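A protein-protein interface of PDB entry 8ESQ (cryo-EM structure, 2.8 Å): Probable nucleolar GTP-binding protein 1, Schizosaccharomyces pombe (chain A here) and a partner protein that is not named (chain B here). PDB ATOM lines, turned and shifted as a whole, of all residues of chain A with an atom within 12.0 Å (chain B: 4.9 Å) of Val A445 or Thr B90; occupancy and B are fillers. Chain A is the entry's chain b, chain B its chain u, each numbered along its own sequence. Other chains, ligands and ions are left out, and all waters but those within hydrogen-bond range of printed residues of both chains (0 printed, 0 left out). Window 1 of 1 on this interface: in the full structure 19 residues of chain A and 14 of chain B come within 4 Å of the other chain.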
ATOM      1  N   ARG A 431       6.687  -3.084  13.375  1.00  0.00           N
ATOM      2  CA  ARG A 431       6.170  -3.454  12.067  1.00  0.00           C
ATOM      3  C   ARG A 431       5.633  -4.883  12.084  1.00  0.00           C
ATOM      4  O   ARG A 431       5.798  -5.631  13.049  1.00  0.00           O
ATOM      5  CB  ARG A 431       7.258  -3.306  11.003  1.00  0.00           C
ATOM      6  N   MET A 432       4.981  -5.259  10.987  1.00  0.00           N
ATOM      7  CA  MET A 432       4.400  -6.581  10.832  1.00  0.00           C
ATOM      8  C   MET A 432       4.826  -7.180   9.501  1.00  0.00           C
ATOM      9  O   MET A 432       5.136  -6.448   8.555  1.00  0.00           O
ATOM     10  CB  MET A 432       2.868  -6.529  10.903  1.00  0.00           C
ATOM     11  N   PRO A 433       4.850  -8.510   9.399  1.00  0.00           N
ATOM     12  CA  PRO A 433       5.279  -9.150   8.145  1.00  0.00           C
ATOM     13  C   PRO A 433       4.260  -8.914   7.039  1.00  0.00           C
ATOM     14  O   PRO A 433       3.083  -9.252   7.180  1.00  0.00           O
ATOM     15  CB  PRO A 433       5.377 -10.633   8.521  1.00  0.00           C
ATOM     16  N   GLU A 434       4.721  -8.326   5.934  1.00  0.00           N
ATOM     17  CA  GLU A 434       3.830  -8.073   4.806  1.00  0.00           C
ATOM     18  C   GLU A 434       3.494  -9.363   4.068  1.00  0.00           C
ATOM     19  O   GLU A 434       2.342  -9.573   3.667  1.00  0.00           O
ATOM     20  CB  GLU A 434       4.462  -7.059   3.855  1.00  0.00           C
ATOM     21  N   LEU A 435       4.480 -10.234   3.874  1.00  0.00           N
ATOM     22  CA  LEU A 435       4.267 -11.510   3.208  1.00  0.00           C
ATOM     23  C   LEU A 435       5.207 -12.539   3.815  1.00  0.00           C
ATOM     24  O   LEU A 435       6.366 -12.233   4.099  1.00  0.00           O
ATOM     25  CB  LEU A 435       4.497 -11.402   1.697  1.00  0.00           C
ATOM     26  N   LEU A 436       4.702 -13.756   4.015  1.00  0.00           N
ATOM     27  CA  LEU A 436       5.486 -14.824   4.616  1.00  0.00           C
ATOM     28  C   LEU A 436       5.182 -16.144   3.926  1.00  0.00           C
ATOM     29  O   LEU A 436       4.017 -16.471   3.682  1.00  0.00           O
ATOM     30  CB  LEU A 436       5.207 -14.946   6.120  1.00  0.00           C
ATOM     31  N   ASP A 437       6.241 -16.896   3.620  1.00  0.00           N
ATOM     32  CA  ASP A 437       6.131 -18.222   3.009  1.00  0.00           C
ATOM     33  C   ASP A 437       5.324 -18.177   1.714  1.00  0.00           C
ATOM     34  O   ASP A 437       4.559 -19.092   1.399  1.00  0.00           O
ATOM     35  CB  ASP A 437       5.531 -19.230   3.993  1.00  0.00           C
ATOM     36  N   GLY A 438       5.499 -17.101   0.953  1.00  0.00           N
ATOM     37  CA  GLY A 438       4.775 -16.930  -0.288  1.00  0.00           C
ATOM     38  C   GLY A 438       3.350 -16.453  -0.138  1.00  0.00           C
ATOM     39  O   GLY A 438       2.643 -16.340  -1.146  1.00  0.00           O
ATOM     40  N   LYS A 439       2.904 -16.168   1.082  1.00  0.00           N
ATOM     41  CA  LYS A 439       1.552 -15.697   1.343  1.00  0.00           C
ATOM     42  C   LYS A 439       1.611 -14.357   2.063  1.00  0.00           C
ATOM     43  O   LYS A 439       2.405 -14.176   2.992  1.00  0.00           O
ATOM     44  CB  LYS A 439       0.764 -16.708   2.180  1.00  0.00           C
ATOM     45  N   ASN A 440       0.764 -13.425   1.634  1.00  0.00           N
ATOM     46  CA  ASN A 440       0.750 -12.079   2.198  1.00  0.00           C
ATOM     47  C   ASN A 440       0.025 -12.107   3.538  1.00  0.00           C
ATOM     48  O   ASN A 440      -1.199 -12.265   3.587  1.00  0.00           O
ATOM     49  CB  ASN A 440       0.084 -11.103   1.234  1.00  0.00           C
ATOM     50  N   VAL A 441       0.781 -11.955   4.626  1.00  0.00           N
ATOM     51  CA  VAL A 441       0.174 -11.931   5.954  1.00  0.00           C
ATOM     52  C   VAL A 441      -0.733 -10.718   6.103  1.00  0.00           C
ATOM     53  O   VAL A 441      -1.805 -10.798   6.716  1.00  0.00           O
ATOM     54  CB  VAL A 441       1.264 -11.963   7.041  1.00  0.00           C
ATOM     55  N   ALA A 442      -0.321  -9.577   5.547  1.00  0.00           N
ATOM     56  CA  ALA A 442      -1.124  -8.363   5.663  1.00  0.00           C
ATOM     57  C   ALA A 442      -2.470  -8.516   4.967  1.00  0.00           C
ATOM     58  O   ALA A 442      -3.495  -8.042   5.470  1.00  0.00           O
ATOM     59  CB  ALA A 442      -0.356  -7.170   5.094  1.00  0.00           C
ATOM     60  N   ASP A 443      -2.490  -9.178   3.813  1.00  0.00           N
ATOM     61  CA  ASP A 443      -3.708  -9.326   3.029  1.00  0.00           C
ATOM     62  C   ASP A 443      -4.516 -10.560   3.404  1.00  0.00           C
ATOM     63  O   ASP A 443      -5.540 -10.827   2.767  1.00  0.00           O
ATOM     64  CB  ASP A 443      -3.370  -9.373   1.535  1.00  0.00           C
ATOM     65  N   PHE A 444      -4.088 -11.321   4.414  1.00  0.00           N
ATOM     66  CA  PHE A 444      -4.792 -12.536   4.803  1.00  0.00           C
ATOM     67  C   PHE A 444      -4.877 -12.725   6.314  1.00  0.00           C
ATOM     68  O   PHE A 444      -5.081 -13.855   6.772  1.00  0.00           O
ATOM     69  CB  PHE A 444      -4.132 -13.759   4.159  1.00  0.00           C
ATOM     70  N   VAL A 445      -4.721 -11.661   7.100  1.00  0.00           N
ATOM     71  CA  VAL A 445      -4.860 -11.716   8.551  1.00  0.00           C
ATOM     72  C   VAL A 445      -6.023 -10.820   8.948  1.00  0.00           C
ATOM     73  O   VAL A 445      -5.969  -9.599   8.756  1.00  0.00           O
ATOM     74  CB  VAL A 445      -3.571 -11.284   9.264  1.00  0.00           C
ATOM     75  N   ASP A 446      -7.058 -11.417   9.527  1.00  0.00           N
ATOM     76  CA  ASP A 446      -8.271 -10.720   9.917  1.00  0.00           C
ATOM     77  C   ASP A 446      -8.392 -10.671  11.433  1.00  0.00           C
ATOM     78  O   ASP A 446      -7.756 -11.458  12.144  1.00  0.00           O
ATOM     79  CB  ASP A 446      -9.510 -11.406   9.323  1.00  0.00           C
ATOM     80  N   PRO A 447      -9.191  -9.740  11.967  1.00  0.00           N
ATOM     81  CA  PRO A 447      -9.368  -9.692  13.428  1.00  0.00           C
ATOM     82  C   PRO A 447      -9.949 -10.970  14.005  1.00  0.00           C
ATOM     83  O   PRO A 447      -9.625 -11.339  15.140  1.00  0.00           O
ATOM     84  CB  PRO A 447     -10.308  -8.496  13.624  1.00  0.00           C
ATOM     85  N   GLU A 448     -10.805 -11.659  13.249  1.00  0.00           N
ATOM     86  CA  GLU A 448     -11.398 -12.908  13.705  1.00  0.00           C
ATOM     87  C   GLU A 448     -10.485 -14.110  13.499  1.00  0.00           C
ATOM     88  O   GLU A 448     -10.848 -15.217  13.913  1.00  0.00           O
ATOM     89  CB  GLU A 448     -12.729 -13.149  12.989  1.00  0.00           C
ATOM     90  N   ILE A 449      -9.321 -13.923  12.871  1.00  0.00           N
ATOM     91  CA  ILE A 449      -8.412 -15.040  12.627  1.00  0.00           C
ATOM     92  C   ILE A 449      -7.885 -15.617  13.934  1.00  0.00           C
ATOM     93  O   ILE A 449      -7.483 -16.787  13.986  1.00  0.00           O
ATOM     94  CB  ILE A 449      -7.258 -14.599  11.705  1.00  0.00           C
ATOM     95  N   GLU A 450      -7.860 -14.814  15.002  1.00  0.00           N
ATOM     96  CA  GLU A 450      -7.399 -15.314  16.294  1.00  0.00           C
ATOM     97  C   GLU A 450      -8.266 -16.471  16.773  1.00  0.00           C
ATOM     98  O   GLU A 450      -7.756 -17.533  17.149  1.00  0.00           O
ATOM     99  CB  GLU A 450      -7.393 -14.181  17.321  1.00  0.00           C
ATOM    100  N   ALA A 451      -9.586 -16.283  16.766  1.00  0.00           N
ATOM    101  CA  ALA A 451     -10.493 -17.370  17.112  1.00  0.00           C
ATOM    102  C   ALA A 451     -10.645 -18.368  15.972  1.00  0.00           C
ATOM    103  O   ALA A 451     -10.904 -19.550  16.222  1.00  0.00           O
ATOM    104  CB  ALA A 451     -11.861 -16.812  17.507  1.00  0.00           C
ATOM    105  N   LYS A 452     -10.496 -17.913  14.725  1.00  0.00           N
ATOM    106  CA  LYS A 452     -10.641 -18.814  13.586  1.00  0.00           C
ATOM    107  C   LYS A 452      -9.570 -19.897  13.598  1.00  0.00           C
ATOM    108  O   LYS A 452      -9.861 -21.067  13.324  1.00  0.00           O
ATOM    109  CB  LYS A 452     -10.586 -18.021  12.279  1.00  0.00           C
ATOM    110  N   LEU A 453      -8.327 -19.528  13.913  1.00  0.00           N
ATOM    111  CA  LEU A 453      -7.246 -20.510  13.940  1.00  0.00           C
ATOM    112  C   LEU A 453      -7.483 -21.565  15.012  1.00  0.00           C
ATOM    113  O   LEU A 453      -7.259 -22.759  14.777  1.00  0.00           O
ATOM    114  CB  LEU A 453      -5.906 -19.808  14.163  1.00  0.00           C
ATOM    115  N   LEU A 454      -7.927 -21.146  16.200  1.00  0.00           N
ATOM    116  CA  LEU A 454      -8.194 -22.102  17.269  1.00  0.00           C
ATOM    117  C   LEU A 454      -9.333 -23.044  16.897  1.00  0.00           C
ATOM    118  O   LEU A 454      -9.239 -24.258  17.111  1.00  0.00           O
ATOM    119  CB  LEU A 454      -8.512 -21.362  18.567  1.00  0.00           C
ATOM    120  N   ALA A 455     -10.419 -22.501  16.340  1.00  0.00           N
ATOM    121  CA  ALA A 455     -11.514 -23.350  15.883  1.00  0.00           C
ATOM    122  C   ALA A 455     -11.074 -24.232  14.723  1.00  0.00           C
ATOM    123  O   ALA A 455     -11.489 -25.393  14.619  1.00  0.00           O
ATOM    124  CB  ALA A 455     -12.713 -22.492  15.483  1.00  0.00           C
ATOM    125  N   LEU A 456     -10.238 -23.692  13.835  1.00  0.00           N
ATOM    126  CA  LEU A 456      -9.717 -24.481  12.725  1.00  0.00           C
ATOM    127  C   LEU A 456      -8.856 -25.637  13.218  1.00  0.00           C
ATOM    128  O   LEU A 456      -8.950 -26.755  12.700  1.00  0.00           O
ATOM    129  CB  LEU A 456      -8.918 -23.583  11.784  1.00  0.00           C
ATOM    130  N   ASP A 457      -8.002 -25.382  14.214  1.00  0.00           N
ATOM    131  CA  ASP A 457      -7.152 -26.440  14.751  1.00  0.00           C
ATOM    132  C   ASP A 457      -7.984 -27.546  15.385  1.00  0.00           C
ATOM    133  O   ASP A 457      -7.668 -28.734  15.237  1.00  0.00           O
ATOM    134  CB  ASP A 457      -6.168 -25.857  15.765  1.00  0.00           C
ATOM    135  N   ARG B  76      -9.065  -9.169   1.044  1.00  0.00           N
ATOM    136  CA  ARG B  76      -9.757  -8.367   2.043  1.00  0.00           C
ATOM    137  C   ARG B  76      -9.591  -6.894   1.694  1.00  0.00           C
ATOM    138  O   ARG B  76      -8.493  -6.341   1.806  1.00  0.00           O
ATOM    139  CB  ARG B  76      -9.211  -8.661   3.436  1.00  0.00           C
ATOM    140  CG  ARG B  76      -9.924  -7.923   4.549  1.00  0.00           C
ATOM    141  CD  ARG B  76      -9.516  -8.483   5.893  1.00  0.00           C
ATOM    142  NE  ARG B  76      -8.079  -8.347   6.095  1.00  0.00           N
ATOM    143  CZ  ARG B  76      -7.224  -9.359   6.126  1.00  0.00           C
ATOM    144  NH1 ARG B  76      -7.627 -10.611   5.975  1.00  0.00           N
ATOM    145  NH2 ARG B  76      -5.931  -9.110   6.311  1.00  0.00           N
ATOM    146  N   VAL B  80      -7.742  -4.038   8.629  1.00  0.00           N
ATOM    147  CA  VAL B  80      -7.928  -4.564   9.974  1.00  0.00           C
ATOM    148  C   VAL B  80      -6.947  -3.882  10.918  1.00  0.00           C
ATOM    149  O   VAL B  80      -5.800  -3.610  10.548  1.00  0.00           O
ATOM    150  CB  VAL B  80      -7.744  -6.095  10.001  1.00  0.00           C
ATOM    151  CG1 VAL B  80      -8.050  -6.653  11.377  1.00  0.00           C
ATOM    152  CG2 VAL B  80      -8.624  -6.751   8.951  1.00  0.00           C
ATOM    153  N   VAL B  86      -3.055 -11.487  17.181  1.00  0.00           N
ATOM    154  CA  VAL B  86      -3.722 -11.860  15.934  1.00  0.00           C
ATOM    155  C   VAL B  86      -2.703 -12.121  14.835  1.00  0.00           C
ATOM    156  O   VAL B  86      -2.781 -13.130  14.122  1.00  0.00           O
ATOM    157  CB  VAL B  86      -4.731 -10.772  15.521  1.00  0.00           C
ATOM    158  CG1 VAL B  86      -5.088 -10.908  14.048  1.00  0.00           C
ATOM    159  CG2 VAL B  86      -5.988 -10.880  16.364  1.00  0.00           C
ATOM    160  N   ILE B  87      -1.731 -11.220  14.680  1.00  0.00           N
ATOM    161  CA  ILE B  87      -0.703 -11.408  13.664  1.00  0.00           C
ATOM    162  C   ILE B  87       0.135 -12.643  13.974  1.00  0.00           C
ATOM    163  O   ILE B  87       0.732 -13.246  13.075  1.00  0.00           O
ATOM    164  CB  ILE B  87       0.161 -10.139  13.530  1.00  0.00           C
ATOM    165  CG1 ILE B  87       0.752 -10.034  12.122  1.00  0.00           C
ATOM    166  CG2 ILE B  87       1.277 -10.122  14.560  1.00  0.00           C
ATOM    167  CD1 ILE B  87      -0.273  -9.786  11.037  1.00  0.00           C
ATOM    168  N   ALA B  88       0.208 -13.030  15.249  1.00  0.00           N
ATOM    169  CA  ALA B  88       0.851 -14.291  15.600  1.00  0.00           C
ATOM    170  C   ALA B  88       0.010 -15.477  15.143  1.00  0.00           C
ATOM    171  O   ALA B  88       0.505 -16.383  14.466  1.00  0.00           O
ATOM    172  CB  ALA B  88       1.097 -14.354  17.108  1.00  0.00           C
ATOM    173  N   THR B  89      -1.283 -15.467  15.479  1.00  0.00           N
ATOM    174  CA  THR B  89      -2.133 -16.628  15.222  1.00  0.00           C
ATOM    175  C   THR B  89      -2.252 -16.926  13.734  1.00  0.00           C
ATOM    176  O   THR B  89      -2.238 -18.092  13.324  1.00  0.00           O
ATOM    177  CB  THR B  89      -3.519 -16.421  15.836  1.00  0.00           C
ATOM    178  OG1 THR B  89      -4.096 -15.208  15.334  1.00  0.00           O
ATOM    179  CG2 THR B  89      -3.438 -16.370  17.356  1.00  0.00           C
ATOM    180  N   THR B  90      -2.378 -15.885  12.907  1.00  0.00           N
ATOM    181  CA  THR B  90      -2.497 -16.111  11.470  1.00  0.00           C
ATOM    182  C   THR B  90      -1.235 -16.755  10.907  1.00  0.00           C
ATOM    183  O   THR B  90      -1.310 -17.595  10.003  1.00  0.00           O
ATOM    184  CB  THR B  90      -2.805 -14.799  10.746  1.00  0.00           C
ATOM    185  OG1 THR B  90      -2.727 -15.004   9.329  1.00  0.00           O
ATOM    186  CG2 THR B  90      -1.818 -13.722  11.145  1.00  0.00           C
ATOM    187  N   LEU B  91      -0.063 -16.370  11.425  1.00  0.00           N
ATOM    188  CA  LEU B  91       1.184 -16.970  10.957  1.00  0.00           C
ATOM    189  C   LEU B  91       1.238 -18.458  11.277  1.00  0.00           C
ATOM    190  O   LEU B  91       1.620 -19.269  10.425  1.00  0.00           O
ATOM    191  CB  LEU B  91       2.382 -16.242  11.565  1.00  0.00           C
ATOM    192  CG  LEU B  91       2.603 -14.812  11.068  1.00  0.00           C
ATOM    193  CD1 LEU B  91       3.718 -14.130  11.846  1.00  0.00           C
ATOM    194  CD2 LEU B  91       2.904 -14.805   9.577  1.00  0.00           C
ATOM    195  N   ASN B  92       0.870 -18.839  12.503  1.00  0.00           N
ATOM    196  CA  ASN B  92       0.698 -20.258  12.800  1.00  0.00           C
ATOM    197  C   ASN B  92      -0.435 -20.856  11.980  1.00  0.00           C
ATOM    198  O   ASN B  92      -0.335 -21.996  11.512  1.00  0.00           O
ATOM    199  CB  ASN B  92       0.466 -20.471  14.297  1.00  0.00           C
ATOM    200  CG  ASN B  92       1.465 -19.721  15.160  1.00  0.00           C
ATOM    201  OD1 ASN B  92       1.806 -18.576  14.887  1.00  0.00           O
ATOM    202  ND2 ASN B  92       1.931 -20.371  16.219  1.00  0.00           N
ATOM    203  N   ALA B  93      -1.518 -20.102  11.780  1.00  0.00           N
ATOM    204  CA  ALA B  93      -2.603 -20.598  10.943  1.00  0.00           C
ATOM    205  C   ALA B  93      -2.140 -20.837   9.512  1.00  0.00           C
ATOM    206  O   ALA B  93      -2.570 -21.807   8.878  1.00  0.00           O
ATOM    207  CB  ALA B  93      -3.780 -19.623  10.962  1.00  0.00           C
ATOM    208  N   MET B  94      -1.258 -19.980   8.994  1.00  0.00           N
ATOM    209  CA  MET B  94      -0.847 -20.093   7.598  1.00  0.00           C
ATOM    210  C   MET B  94      -0.084 -21.388   7.346  1.00  0.00           C
ATOM    211  O   MET B  94      -0.336 -22.084   6.356  1.00  0.00           O
ATOM    212  CB  MET B  94      -0.010 -18.880   7.199  1.00  0.00           C
ATOM    213  CG  MET B  94      -0.859 -17.711   6.750  1.00  0.00           C
ATOM    214  SD  MET B  94      -2.399 -18.289   6.011  1.00  0.00           S
ATOM    215  CE  MET B  94      -3.230 -16.737   5.714  1.00  0.00           C
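The backbone carbonyl oxygen (O) of Ala A442 sits at hydrogen-bond distance from the guanidinium group (NH2) of Arg B76.
The backbone carbonyl oxygen of Val A445 lies within hydrogen-bond range of the guanidinium group of Arg B76, 2.5 Å away.
The backbone NH (N) of Phe A444 sits close to the guanidinium group (NH2) of Arg B76, at 3.4 Å.
Asp A443 touches Arg B76.
CB of Phe A444 touches CE of Met B94, at 3.5 Å.
Val A445 touches Val B80 (O to CG2, 3.9 Å).
Asp A446 touches Arg B76.
Asp A446 touches Val B86 (O to CG1, 3.3 Å).
O of Pro A447 touches CG2 of Val B86 (3.9 Å).
Ile A449 touches Thr B89.
CG2 of Val B86 touches CB of Glu A450, 3.7 Å away.
Glu A450 touches Thr B89.
Leu A453 touches Ala B93.
Of the 11 printed residues of chain B, 7 touch a printed residue of chain A.
Printed residues of chain B that touch a printed residue of chain A: Arg B76, Val B80, Val B86, Thr B89, Thr B90, Ala B93 and Met B94.
Hydrophobic or aromatic side chains of chain B that line the printed part of chain A: Val B80, Val B86, Ala B93 and Met B94.
Along chain A the printed residues that touch a printed residue of chain B span positions 442 to 453.
Among the printed residues, 16 pairs touch across the chains.
Among the printed residues, no Asp or Glu carboxylate lies within 4 Å of a Lys or Arg side-chain nitrogen of the other chain.
Of the printed residues of chain B, Val A445 touches Arg B76 (2.5 Å), Val B80 (3.9 Å) and Thr B90 (3.5 Å).
Thr B90 touches just these residues of chain A: Phe A444 and Val A445.
Val B86 touches just these residues of chain A: Asp A446, Pro A447 and Glu A450.
No residue of chain A comes within 4 Å of Ala B88.
Of chain A, only Ile A449 and Glu A450 come within 4 Å of Thr B89.
No residue of chain A comes within 4 Å of Leu B91.
No residue of chain A comes within 4 Å of Asn B92.
Ala B93 touches one residue of chain A.
Of the printed residues of chain A, Met B94 touches Phe A444 (3.5 Å).
Of the printed residues of chain B, Leu A453 touches Ala B93 (3.8 Å).
Of the printed residues of chain B, Asp A446 touches Arg B76 (3.7 Å) and Val B86 (3.3 Å).
Of the printed residues of chain A, Arg B76 touches Ala A442 (2.8 Å), Asp A443 (3.5 Å), Phe A444 (3.4 Å), Val A445 (2.5 Å) and Asp A446 (3.7 Å).
Of the printed residues of chain B, Ile A449 touches Thr B89.
Lys A452 touches none of the printed residues of chain B.
Gly A438 touches none of the printed residues of chain B.
The nearest residue of chain A that does not touch Thr B90 is Ile A449 (4.6 Å).
The nearest printed residue of chain B that does not touch Leu A453 is Thr B89 (4.1 Å).
O of Glu A434 sits at hydrogen-bond distance from N of Ala A442 (3.3 Å).
The backbone carbonyl oxygen of Val B86 sits at hydrogen-bond distance from the side-chain hydroxyl of Thr B89 (2.7 Å).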
